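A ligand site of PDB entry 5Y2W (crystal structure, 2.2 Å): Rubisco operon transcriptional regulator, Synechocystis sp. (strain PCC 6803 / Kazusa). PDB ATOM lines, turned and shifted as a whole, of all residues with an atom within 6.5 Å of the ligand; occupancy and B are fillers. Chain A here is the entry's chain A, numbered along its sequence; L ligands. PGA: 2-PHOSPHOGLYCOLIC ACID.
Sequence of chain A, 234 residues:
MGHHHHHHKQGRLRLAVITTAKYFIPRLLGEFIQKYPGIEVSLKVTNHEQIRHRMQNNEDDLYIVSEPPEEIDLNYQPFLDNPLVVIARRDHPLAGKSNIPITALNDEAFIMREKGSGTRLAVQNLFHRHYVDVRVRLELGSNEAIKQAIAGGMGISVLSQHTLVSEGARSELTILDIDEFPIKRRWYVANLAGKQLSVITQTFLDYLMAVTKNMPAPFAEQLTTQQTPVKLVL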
ATOM      1  N   ILE A  18       7.322 -22.322 -13.303  1.00  0.00           N
ATOM      2  CA  ILE A  18       6.297 -22.893 -14.170  1.00  0.00           C
ATOM      3  C   ILE A  18       5.652 -21.826 -15.072  1.00  0.00           C
ATOM      4  O   ILE A  18       5.695 -20.641 -14.776  1.00  0.00           O
ATOM      5  CB  ILE A  18       5.253 -23.652 -13.372  1.00  0.00           C
ATOM      6  CG1 ILE A  18       4.694 -22.755 -12.269  1.00  0.00           C
ATOM      7  CG2 ILE A  18       5.859 -24.951 -12.861  1.00  0.00           C
ATOM      8  CD1 ILE A  18       3.380 -23.221 -11.742  1.00  0.00           C
ATOM      9  N   THR A  19       5.012 -22.266 -16.148  1.00  0.00           N
ATOM     10  CA  THR A  19       4.641 -21.350 -17.208  1.00  0.00           C
ATOM     11  C   THR A  19       3.756 -20.234 -16.704  1.00  0.00           C
ATOM     12  O   THR A  19       3.881 -19.100 -17.133  1.00  0.00           O
ATOM     13  CB  THR A  19       3.873 -22.075 -18.332  1.00  0.00           C
ATOM     14  OG1 THR A  19       2.773 -22.775 -17.729  1.00  0.00           O
ATOM     15  CG2 THR A  19       4.773 -23.041 -19.075  1.00  0.00           C
ATOM     16  N   THR A  20       2.879 -20.548 -15.782  1.00  0.00           N
ATOM     17  CA  THR A  20       1.838 -19.615 -15.411  1.00  0.00           C
ATOM     18  C   THR A  20       2.356 -18.448 -14.530  1.00  0.00           C
ATOM     19  O   THR A  20       1.632 -17.479 -14.236  1.00  0.00           O
ATOM     20  CB  THR A  20       0.733 -20.385 -14.667  1.00  0.00           C
ATOM     21  OG1 THR A  20       1.307 -21.168 -13.590  1.00  0.00           O
ATOM     22  CG2 THR A  20       0.089 -21.328 -15.625  1.00  0.00           C
ATOM     23  N   ALA A  21       3.586 -18.591 -14.063  1.00  0.00           N
ATOM     24  CA  ALA A  21       4.250 -17.597 -13.208  1.00  0.00           C
ATOM     25  C   ALA A  21       5.121 -16.609 -13.962  1.00  0.00           C
ATOM     26  O   ALA A  21       5.785 -15.818 -13.338  1.00  0.00           O
ATOM     27  CB  ALA A  21       5.097 -18.323 -12.169  1.00  0.00           C
ATOM     28  N   THR A  46       9.369 -22.892 -17.551  1.00  0.00           N
ATOM     29  CA  THR A  46       9.107 -24.201 -18.068  1.00  0.00           C
ATOM     30  C   THR A  46       7.814 -24.800 -17.524  1.00  0.00           C
ATOM     31  O   THR A  46       7.095 -24.189 -16.743  1.00  0.00           O
ATOM     32  CB  THR A  46      10.349 -25.073 -17.721  1.00  0.00           C
ATOM     33  OG1 THR A  46      10.296 -26.271 -18.507  1.00  0.00           O
ATOM     34  CG2 THR A  46      10.345 -25.469 -16.292  1.00  0.00           C
ATOM     35  N   ASN A  47       7.503 -26.034 -17.955  1.00  0.00           N
ATOM     36  CA  ASN A  47       6.424 -26.801 -17.376  1.00  0.00           C
ATOM     37  C   ASN A  47       6.944 -27.730 -16.300  1.00  0.00           C
ATOM     38  O   ASN A  47       8.117 -27.762 -16.027  1.00  0.00           O
ATOM     39  CB  ASN A  47       5.620 -27.527 -18.496  1.00  0.00           C
ATOM     40  CG  ASN A  47       6.346 -28.750 -19.061  1.00  0.00           C
ATOM     41  OD1 ASN A  47       7.295 -29.272 -18.483  1.00  0.00           O
ATOM     42  ND2 ASN A  47       5.889 -29.203 -20.222  1.00  0.00           N
ATOM     43  N   HIS A  48       6.054 -28.432 -15.626  1.00  0.00           N
ATOM     44  CA  HIS A  48       6.476 -29.184 -14.444  1.00  0.00           C
ATOM     45  C   HIS A  48       7.433 -30.316 -14.800  1.00  0.00           C
ATOM     46  O   HIS A  48       8.355 -30.622 -14.041  1.00  0.00           O
ATOM     47  CB  HIS A  48       5.276 -29.732 -13.682  1.00  0.00           C
ATOM     48  CG  HIS A  48       4.665 -28.761 -12.723  1.00  0.00           C
ATOM     49  ND1 HIS A  48       3.654 -27.881 -13.074  1.00  0.00           N
ATOM     50  CD2 HIS A  48       4.885 -28.572 -11.394  1.00  0.00           C
ATOM     51  CE1 HIS A  48       3.287 -27.185 -12.006  1.00  0.00           C
ATOM     52  NE2 HIS A  48       4.035 -27.566 -10.981  1.00  0.00           N
ATOM     53  N   GLU A  49       7.223 -30.952 -15.947  1.00  0.00           N
ATOM     54  CA  GLU A  49       8.061 -32.066 -16.293  1.00  0.00           C
ATOM     55  C   GLU A  49       9.457 -31.536 -16.516  1.00  0.00           C
ATOM     56  O   GLU A  49      10.421 -32.071 -16.010  1.00  0.00           O
ATOM     57  CB  GLU A  49       7.543 -32.788 -17.547  1.00  0.00           C
ATOM     58  CG  GLU A  49       8.384 -33.986 -17.934  1.00  0.00           C
ATOM     59  CD  GLU A  49       8.648 -34.002 -19.428  1.00  0.00           C
ATOM     60  OE1 GLU A  49       7.769 -34.493 -20.171  1.00  0.00           O
ATOM     61  OE2 GLU A  49       9.723 -33.496 -19.850  1.00  0.00           O
ATOM     62  N   VAL A  65       6.755 -23.976  -8.409  1.00  0.00           N
ATOM     63  CA  VAL A  65       5.957 -25.098  -8.835  1.00  0.00           C
ATOM     64  C   VAL A  65       4.613 -25.043  -8.108  1.00  0.00           C
ATOM     65  O   VAL A  65       4.497 -24.389  -7.067  1.00  0.00           O
ATOM     66  CB  VAL A  65       6.653 -26.403  -8.519  1.00  0.00           C
ATOM     67  CG1 VAL A  65       7.997 -26.414  -9.215  1.00  0.00           C
ATOM     68  CG2 VAL A  65       6.792 -26.596  -6.997  1.00  0.00           C
ATOM     69  N   SER A  66       3.577 -25.656  -8.696  1.00  0.00           N
ATOM     70  CA  SER A  66       2.302 -25.937  -8.027  1.00  0.00           C
ATOM     71  C   SER A  66       2.172 -27.356  -7.427  1.00  0.00           C
ATOM     72  O   SER A  66       1.490 -27.562  -6.449  1.00  0.00           O
ATOM     73  CB  SER A  66       1.153 -25.732  -9.012  1.00  0.00           C
ATOM     74  OG  SER A  66       1.116 -24.392  -9.379  1.00  0.00           O
ATOM     75  N   GLU A  67       2.742 -28.318  -8.110  1.00  0.00           N
ATOM     76  CA  GLU A  67       2.725 -29.713  -7.720  1.00  0.00           C
ATOM     77  C   GLU A  67       4.213 -30.134  -7.575  1.00  0.00           C
ATOM     78  O   GLU A  67       4.931 -30.216  -8.553  1.00  0.00           O
ATOM     79  CB  GLU A  67       1.989 -30.598  -8.734  1.00  0.00           C
ATOM     80  CG  GLU A  67       1.801 -32.005  -8.204  1.00  0.00           C
ATOM     81  CD  GLU A  67       1.263 -33.024  -9.185  1.00  0.00           C
ATOM     82  OE1 GLU A  67       1.097 -32.748 -10.404  1.00  0.00           O
ATOM     83  OE2 GLU A  67       0.999 -34.147  -8.709  1.00  0.00           O
ATOM     84  N   ASN A  82      -3.026 -20.608  -6.825  1.00  0.00           N
ATOM     85  CA  ASN A  82      -2.975 -20.772  -8.244  1.00  0.00           C
ATOM     86  C   ASN A  82      -4.228 -21.497  -8.711  1.00  0.00           C
ATOM     87  O   ASN A  82      -4.183 -22.656  -9.126  1.00  0.00           O
ATOM     88  CB  ASN A  82      -1.726 -21.560  -8.591  1.00  0.00           C
ATOM     89  CG  ASN A  82      -1.572 -21.723 -10.099  1.00  0.00           C
ATOM     90  OD1 ASN A  82      -2.034 -20.879 -10.914  1.00  0.00           O
ATOM     91  ND2 ASN A  82      -0.952 -22.825 -10.475  1.00  0.00           N
ATOM     92  N   LEU A  84      -6.898 -22.965 -10.987  1.00  0.00           N
ATOM     93  CA  LEU A  84      -7.115 -23.330 -12.383  1.00  0.00           C
ATOM     94  C   LEU A  84      -8.610 -23.258 -12.740  1.00  0.00           C
ATOM     95  O   LEU A  84      -9.454 -23.822 -12.025  1.00  0.00           O
ATOM     96  CB  LEU A  84      -6.660 -24.744 -12.617  1.00  0.00           C
ATOM     97  CG  LEU A  84      -5.229 -25.115 -12.226  1.00  0.00           C
ATOM     98  CD1 LEU A  84      -4.911 -26.501 -12.786  1.00  0.00           C
ATOM     99  CD2 LEU A  84      -4.173 -24.140 -12.678  1.00  0.00           C
ATOM    100  N   ARG A 113      -3.095 -28.746 -22.925  1.00  0.00           N
ATOM    101  CA  ARG A 113      -1.688 -28.424 -22.891  1.00  0.00           C
ATOM    102  C   ARG A 113      -0.881 -29.662 -23.320  1.00  0.00           C
ATOM    103  O   ARG A 113      -1.425 -30.781 -23.391  1.00  0.00           O
ATOM    104  CB  ARG A 113      -1.290 -28.045 -21.428  1.00  0.00           C
ATOM    105  CG  ARG A 113      -1.707 -26.662 -20.985  1.00  0.00           C
ATOM    106  CD  ARG A 113      -0.803 -25.579 -21.515  1.00  0.00           C
ATOM    107  NE  ARG A 113       0.568 -25.876 -21.124  1.00  0.00           N
ATOM    108  CZ  ARG A 113       1.133 -25.583 -19.946  1.00  0.00           C
ATOM    109  NH1 ARG A 113       2.369 -26.057 -19.687  1.00  0.00           N
ATOM    110  NH2 ARG A 113       0.465 -24.854 -19.036  1.00  0.00           N
ATOM    111  N   GLU A 114       0.410 -29.463 -23.594  1.00  0.00           N
ATOM    112  CA  GLU A 114       1.389 -30.551 -23.890  1.00  0.00           C
ATOM    113  C   GLU A 114       1.507 -31.515 -22.708  1.00  0.00           C
ATOM    114  O   GLU A 114       1.280 -31.119 -21.549  1.00  0.00           O
ATOM    115  CB  GLU A 114       2.760 -29.977 -24.208  1.00  0.00           C
ATOM    116  CG  GLU A 114       3.616 -29.471 -23.031  1.00  0.00           C
ATOM    117  CD  GLU A 114       3.124 -28.164 -22.385  1.00  0.00           C
ATOM    118  OE1 GLU A 114       3.730 -27.764 -21.352  1.00  0.00           O
ATOM    119  OE2 GLU A 114       2.100 -27.557 -22.853  1.00  0.00           O
ATOM    120  N   GLY A 116       3.390 -33.446 -20.000  1.00  0.00           N
ATOM    121  CA  GLY A 116       4.357 -32.809 -19.103  1.00  0.00           C
ATOM    122  C   GLY A 116       3.834 -31.574 -18.405  1.00  0.00           C
ATOM    123  O   GLY A 116       4.439 -31.072 -17.449  1.00  0.00           O
ATOM    124  N   SER A 117       2.706 -31.039 -18.885  1.00  0.00           N
ATOM    125  CA  SER A 117       2.109 -29.911 -18.194  1.00  0.00           C
ATOM    126  C   SER A 117       1.444 -30.396 -16.910  1.00  0.00           C
ATOM    127  O   SER A 117       0.692 -31.339 -16.934  1.00  0.00           O
ATOM    128  CB  SER A 117       1.055 -29.267 -19.092  1.00  0.00           C
ATOM    129  OG  SER A 117       0.175 -28.510 -18.318  1.00  0.00           O
ATOM    130  N   GLY A 118       1.700 -29.740 -15.778  1.00  0.00           N
ATOM    131  CA  GLY A 118       0.948 -30.041 -14.548  1.00  0.00           C
ATOM    132  C   GLY A 118      -0.486 -29.586 -14.643  1.00  0.00           C
ATOM    133  O   GLY A 118      -1.370 -30.136 -13.981  1.00  0.00           O
ATOM    134  N   THR A 119      -0.720 -28.582 -15.499  1.00  0.00           N
ATOM    135  CA  THR A 119      -2.089 -28.103 -15.705  1.00  0.00           C
ATOM    136  C   THR A 119      -2.880 -29.253 -16.269  1.00  0.00           C
ATOM    137  O   THR A 119      -3.916 -29.620 -15.698  1.00  0.00           O
ATOM    138  CB  THR A 119      -2.177 -26.883 -16.634  1.00  0.00           C
ATOM    139  OG1 THR A 119      -1.539 -25.786 -16.020  1.00  0.00           O
ATOM    140  CG2 THR A 119      -3.634 -26.477 -16.932  1.00  0.00           C
ATOM    141  N   ARG A 120      -2.371 -29.828 -17.373  1.00  0.00           N
ATOM    142  CA  ARG A 120      -2.993 -30.992 -18.025  1.00  0.00           C
ATOM    143  C   ARG A 120      -3.187 -32.166 -17.029  1.00  0.00           C
ATOM    144  O   ARG A 120      -4.259 -32.764 -16.970  1.00  0.00           O
ATOM    145  CB  ARG A 120      -2.103 -31.402 -19.178  1.00  0.00           C
ATOM    146  CG  ARG A 120      -2.633 -32.530 -20.039  1.00  0.00           C
ATOM    147  CD  ARG A 120      -1.537 -33.019 -20.951  1.00  0.00           C
ATOM    148  NE  ARG A 120      -1.849 -34.313 -21.585  1.00  0.00           N
ATOM    149  CZ  ARG A 120      -1.955 -34.522 -22.901  1.00  0.00           C
ATOM    150  NH1 ARG A 120      -2.241 -35.742 -23.347  1.00  0.00           N
ATOM    151  NH2 ARG A 120      -1.783 -33.544 -23.799  1.00  0.00           N
ATOM    152  N   ASN A 143       0.231 -21.791 -22.690  1.00  0.00           N
ATOM    153  CA  ASN A 143      -0.987 -21.099 -22.237  1.00  0.00           C
ATOM    154  C   ASN A 143      -1.474 -20.024 -23.207  1.00  0.00           C
ATOM    155  O   ASN A 143      -2.683 -19.814 -23.350  1.00  0.00           O
ATOM    156  CB  ASN A 143      -0.824 -20.522 -20.845  1.00  0.00           C
ATOM    157  CG  ASN A 143      -0.459 -21.587 -19.811  1.00  0.00           C
ATOM    158  OD1 ASN A 143      -1.221 -22.532 -19.533  1.00  0.00           O
ATOM    159  ND2 ASN A 143       0.740 -21.463 -19.257  1.00  0.00           N
ATOM    160  N   SER A 160      -4.508 -21.800 -15.523  1.00  0.00           N
ATOM    161  CA  SER A 160      -4.327 -20.916 -14.373  1.00  0.00           C
ATOM    162  C   SER A 160      -4.986 -19.613 -14.619  1.00  0.00           C
ATOM    163  O   SER A 160      -4.785 -18.987 -15.659  1.00  0.00           O
ATOM    164  CB  SER A 160      -2.850 -20.626 -14.110  1.00  0.00           C
ATOM    165  OG  SER A 160      -2.751 -19.742 -13.014  1.00  0.00           O
ATOM    166  N   HIS A 162      -3.997 -17.013 -13.377  1.00  0.00           N
ATOM    167  CA  HIS A 162      -2.931 -16.010 -13.554  1.00  0.00           C
ATOM    168  C   HIS A 162      -2.694 -15.721 -15.022  1.00  0.00           C
ATOM    169  O   HIS A 162      -2.095 -14.699 -15.324  1.00  0.00           O
ATOM    170  CB  HIS A 162      -1.618 -16.471 -12.925  1.00  0.00           C
ATOM    171  CG  HIS A 162      -1.709 -16.658 -11.444  1.00  0.00           C
ATOM    172  ND1 HIS A 162      -1.856 -15.592 -10.580  1.00  0.00           N
ATOM    173  CD2 HIS A 162      -1.710 -17.758 -10.660  1.00  0.00           C
ATOM    174  CE1 HIS A 162      -1.958 -16.034  -9.336  1.00  0.00           C
ATOM    175  NE2 HIS A 162      -1.879 -17.349  -9.364  1.00  0.00           N
ATOM    176  N   ARG A 185      -5.114 -24.905  -6.020  1.00  0.00           N
ATOM    177  CA  ARG A 185      -3.728 -25.252  -6.308  1.00  0.00           C
ATOM    178  C   ARG A 185      -2.937 -24.050  -5.862  1.00  0.00           C
ATOM    179  O   ARG A 185      -3.473 -22.946  -5.723  1.00  0.00           O
ATOM    180  CB  ARG A 185      -3.667 -25.540  -7.803  1.00  0.00           C
ATOM    181  CG  ARG A 185      -2.376 -25.873  -8.447  1.00  0.00           C
ATOM    182  CD  ARG A 185      -2.676 -26.015  -9.956  1.00  0.00           C
ATOM    183  NE  ARG A 185      -1.523 -26.343 -10.815  1.00  0.00           N
ATOM    184  CZ  ARG A 185      -1.015 -27.570 -10.941  1.00  0.00           C
ATOM    185  NH1 ARG A 185      -1.585 -28.571 -10.319  1.00  0.00           N
ATOM    186  NH2 ARG A 185       0.019 -27.800 -11.756  1.00  0.00           N
ATOM    187  N   TRP A 187       0.954 -21.852  -5.768  1.00  0.00           N
ATOM    188  CA  TRP A 187       2.348 -21.727  -6.117  1.00  0.00           C
ATOM    189  C   TRP A 187       3.252 -21.893  -4.883  1.00  0.00           C
ATOM    190  O   TRP A 187       3.060 -21.264  -3.855  1.00  0.00           O
ATOM    191  CB  TRP A 187       2.614 -20.353  -6.742  1.00  0.00           C
ATOM    192  CG  TRP A 187       2.187 -20.175  -8.160  1.00  0.00           C
ATOM    193  CD1 TRP A 187       1.951 -21.140  -9.100  1.00  0.00           C
ATOM    194  CD2 TRP A 187       2.009 -18.936  -8.819  1.00  0.00           C
ATOM    195  NE1 TRP A 187       1.616 -20.569 -10.304  1.00  0.00           N
ATOM    196  CE2 TRP A 187       1.664 -19.221 -10.161  1.00  0.00           C
ATOM    197  CE3 TRP A 187       2.173 -17.601  -8.424  1.00  0.00           C
ATOM    198  CZ2 TRP A 187       1.407 -18.227 -11.077  1.00  0.00           C
ATOM    199  CZ3 TRP A 187       1.893 -16.626  -9.333  1.00  0.00           C
ATOM    200  CH2 TRP A 187       1.555 -16.951 -10.672  1.00  0.00           C
HETATM  201  P   PGA L   1       2.397 -26.290 -16.238  1.00  0.00           P
HETATM  202  O1P PGA L   1       2.190 -25.624 -14.777  1.00  0.00           O
HETATM  203  O2P PGA L   1       3.162 -25.286 -17.038  1.00  0.00           O
HETATM  204  O3P PGA L   1       0.972 -26.580 -16.721  1.00  0.00           O
HETATM  205  O4P PGA L   1       3.332 -27.422 -15.982  1.00  0.00           O
HETATM  206  C2  PGA L   1       1.618 -24.367 -14.479  1.00  0.00           C
HETATM  207  C1  PGA L   1       0.675 -24.417 -13.294  1.00  0.00           C
HETATM  208  O1  PGA L   1       0.092 -23.349 -12.925  1.00  0.00           O
HETATM  209  O2  PGA L   1       0.512 -25.513 -12.717  1.00  0.00           O
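An oxygen (O3P) of the ligand lies within hydrogen-bond range of the backbone NH (N) of Thr 119.
The side-chain hydroxyl of Thr 19 lies within hydrogen-bond range of an oxygen (O2P) of the ligand, at 2.6 Å.
An oxygen (O4P) of the ligand lies within hydrogen-bond range of the backbone NH (N) of His 48.
A ring nitrogen (ND1) of His 48 sits at hydrogen-bond distance from an oxygen (O4P) of the ligand (3.0 Å).
The guanidinium group (NH1) of Arg 113 lies within salt-bridge range of an oxygen (O2P) of the ligand, 2.9 Å away.
The side-chain amide nitrogen (ND2) of Asn 82 is in hydrogen-bond range of an oxygen (O1) of the ligand, at 2.7 Å.
O3P of the ligand lies within hydrogen-bond range of OG of Ser 117, 2.6 Å away.
O3P of the ligand sits at hydrogen-bond distance from OG1 of Thr 119 (2.7 Å).
NH2 of Arg 185 is in salt-bridge range of O2 of the ligand (2.5 Å).
An oxygen (O4P) of the ligand sits at hydrogen-bond distance from the backbone NH (N) of Gly 118, 2.8 Å away.
An oxygen (O1) of the ligand sits at hydrogen-bond distance from the side-chain hydroxyl (OG1) of Thr 20.
The backbone NH (N) of Glu 49 lies within hydrogen-bond range of the side-chain amide oxygen (OD1) of Asn 47 (3.0 Å).
N of Thr 119 is in hydrogen-bond range of OG of Ser 117 (3.0 Å).
The side-chain carboxylate of Glu 114 lies within hydrogen-bond range of the side-chain amide nitrogen of Asn 47, 2.8 Å away.
N of Ser 66 is in hydrogen-bond range of NE2 of His 48, at 3.0 Å.
The side-chain amide oxygen (OD1) of Asn 143 is in hydrogen-bond range of the guanidinium group (NH2) of Arg 113 (2.9 Å).
OG1 of Thr 19 is in hydrogen-bond range of NH2 of Arg 113, at 3.4 Å.
A ring nitrogen (NE2) of His 48 is in hydrogen-bond range of the backbone NH (N) of Glu 67, 3.2 Å away.
The side-chain amide nitrogen (ND2) of Asn 82 lies close to the indole nitrogen (NE1) of Trp 187 (3.4 Å).
CD1 of Ile 18 touches C1 of the ligand, at 3.3 Å.
Asn 47 touches the ligand.
Ser 66 touches the ligand.
Hydrophobic or aromatic side chains that line the ligand: Ile 18 and His 48.
The nearest printed residue that does not touch the ligand is Gly 116 (4.1 Å).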
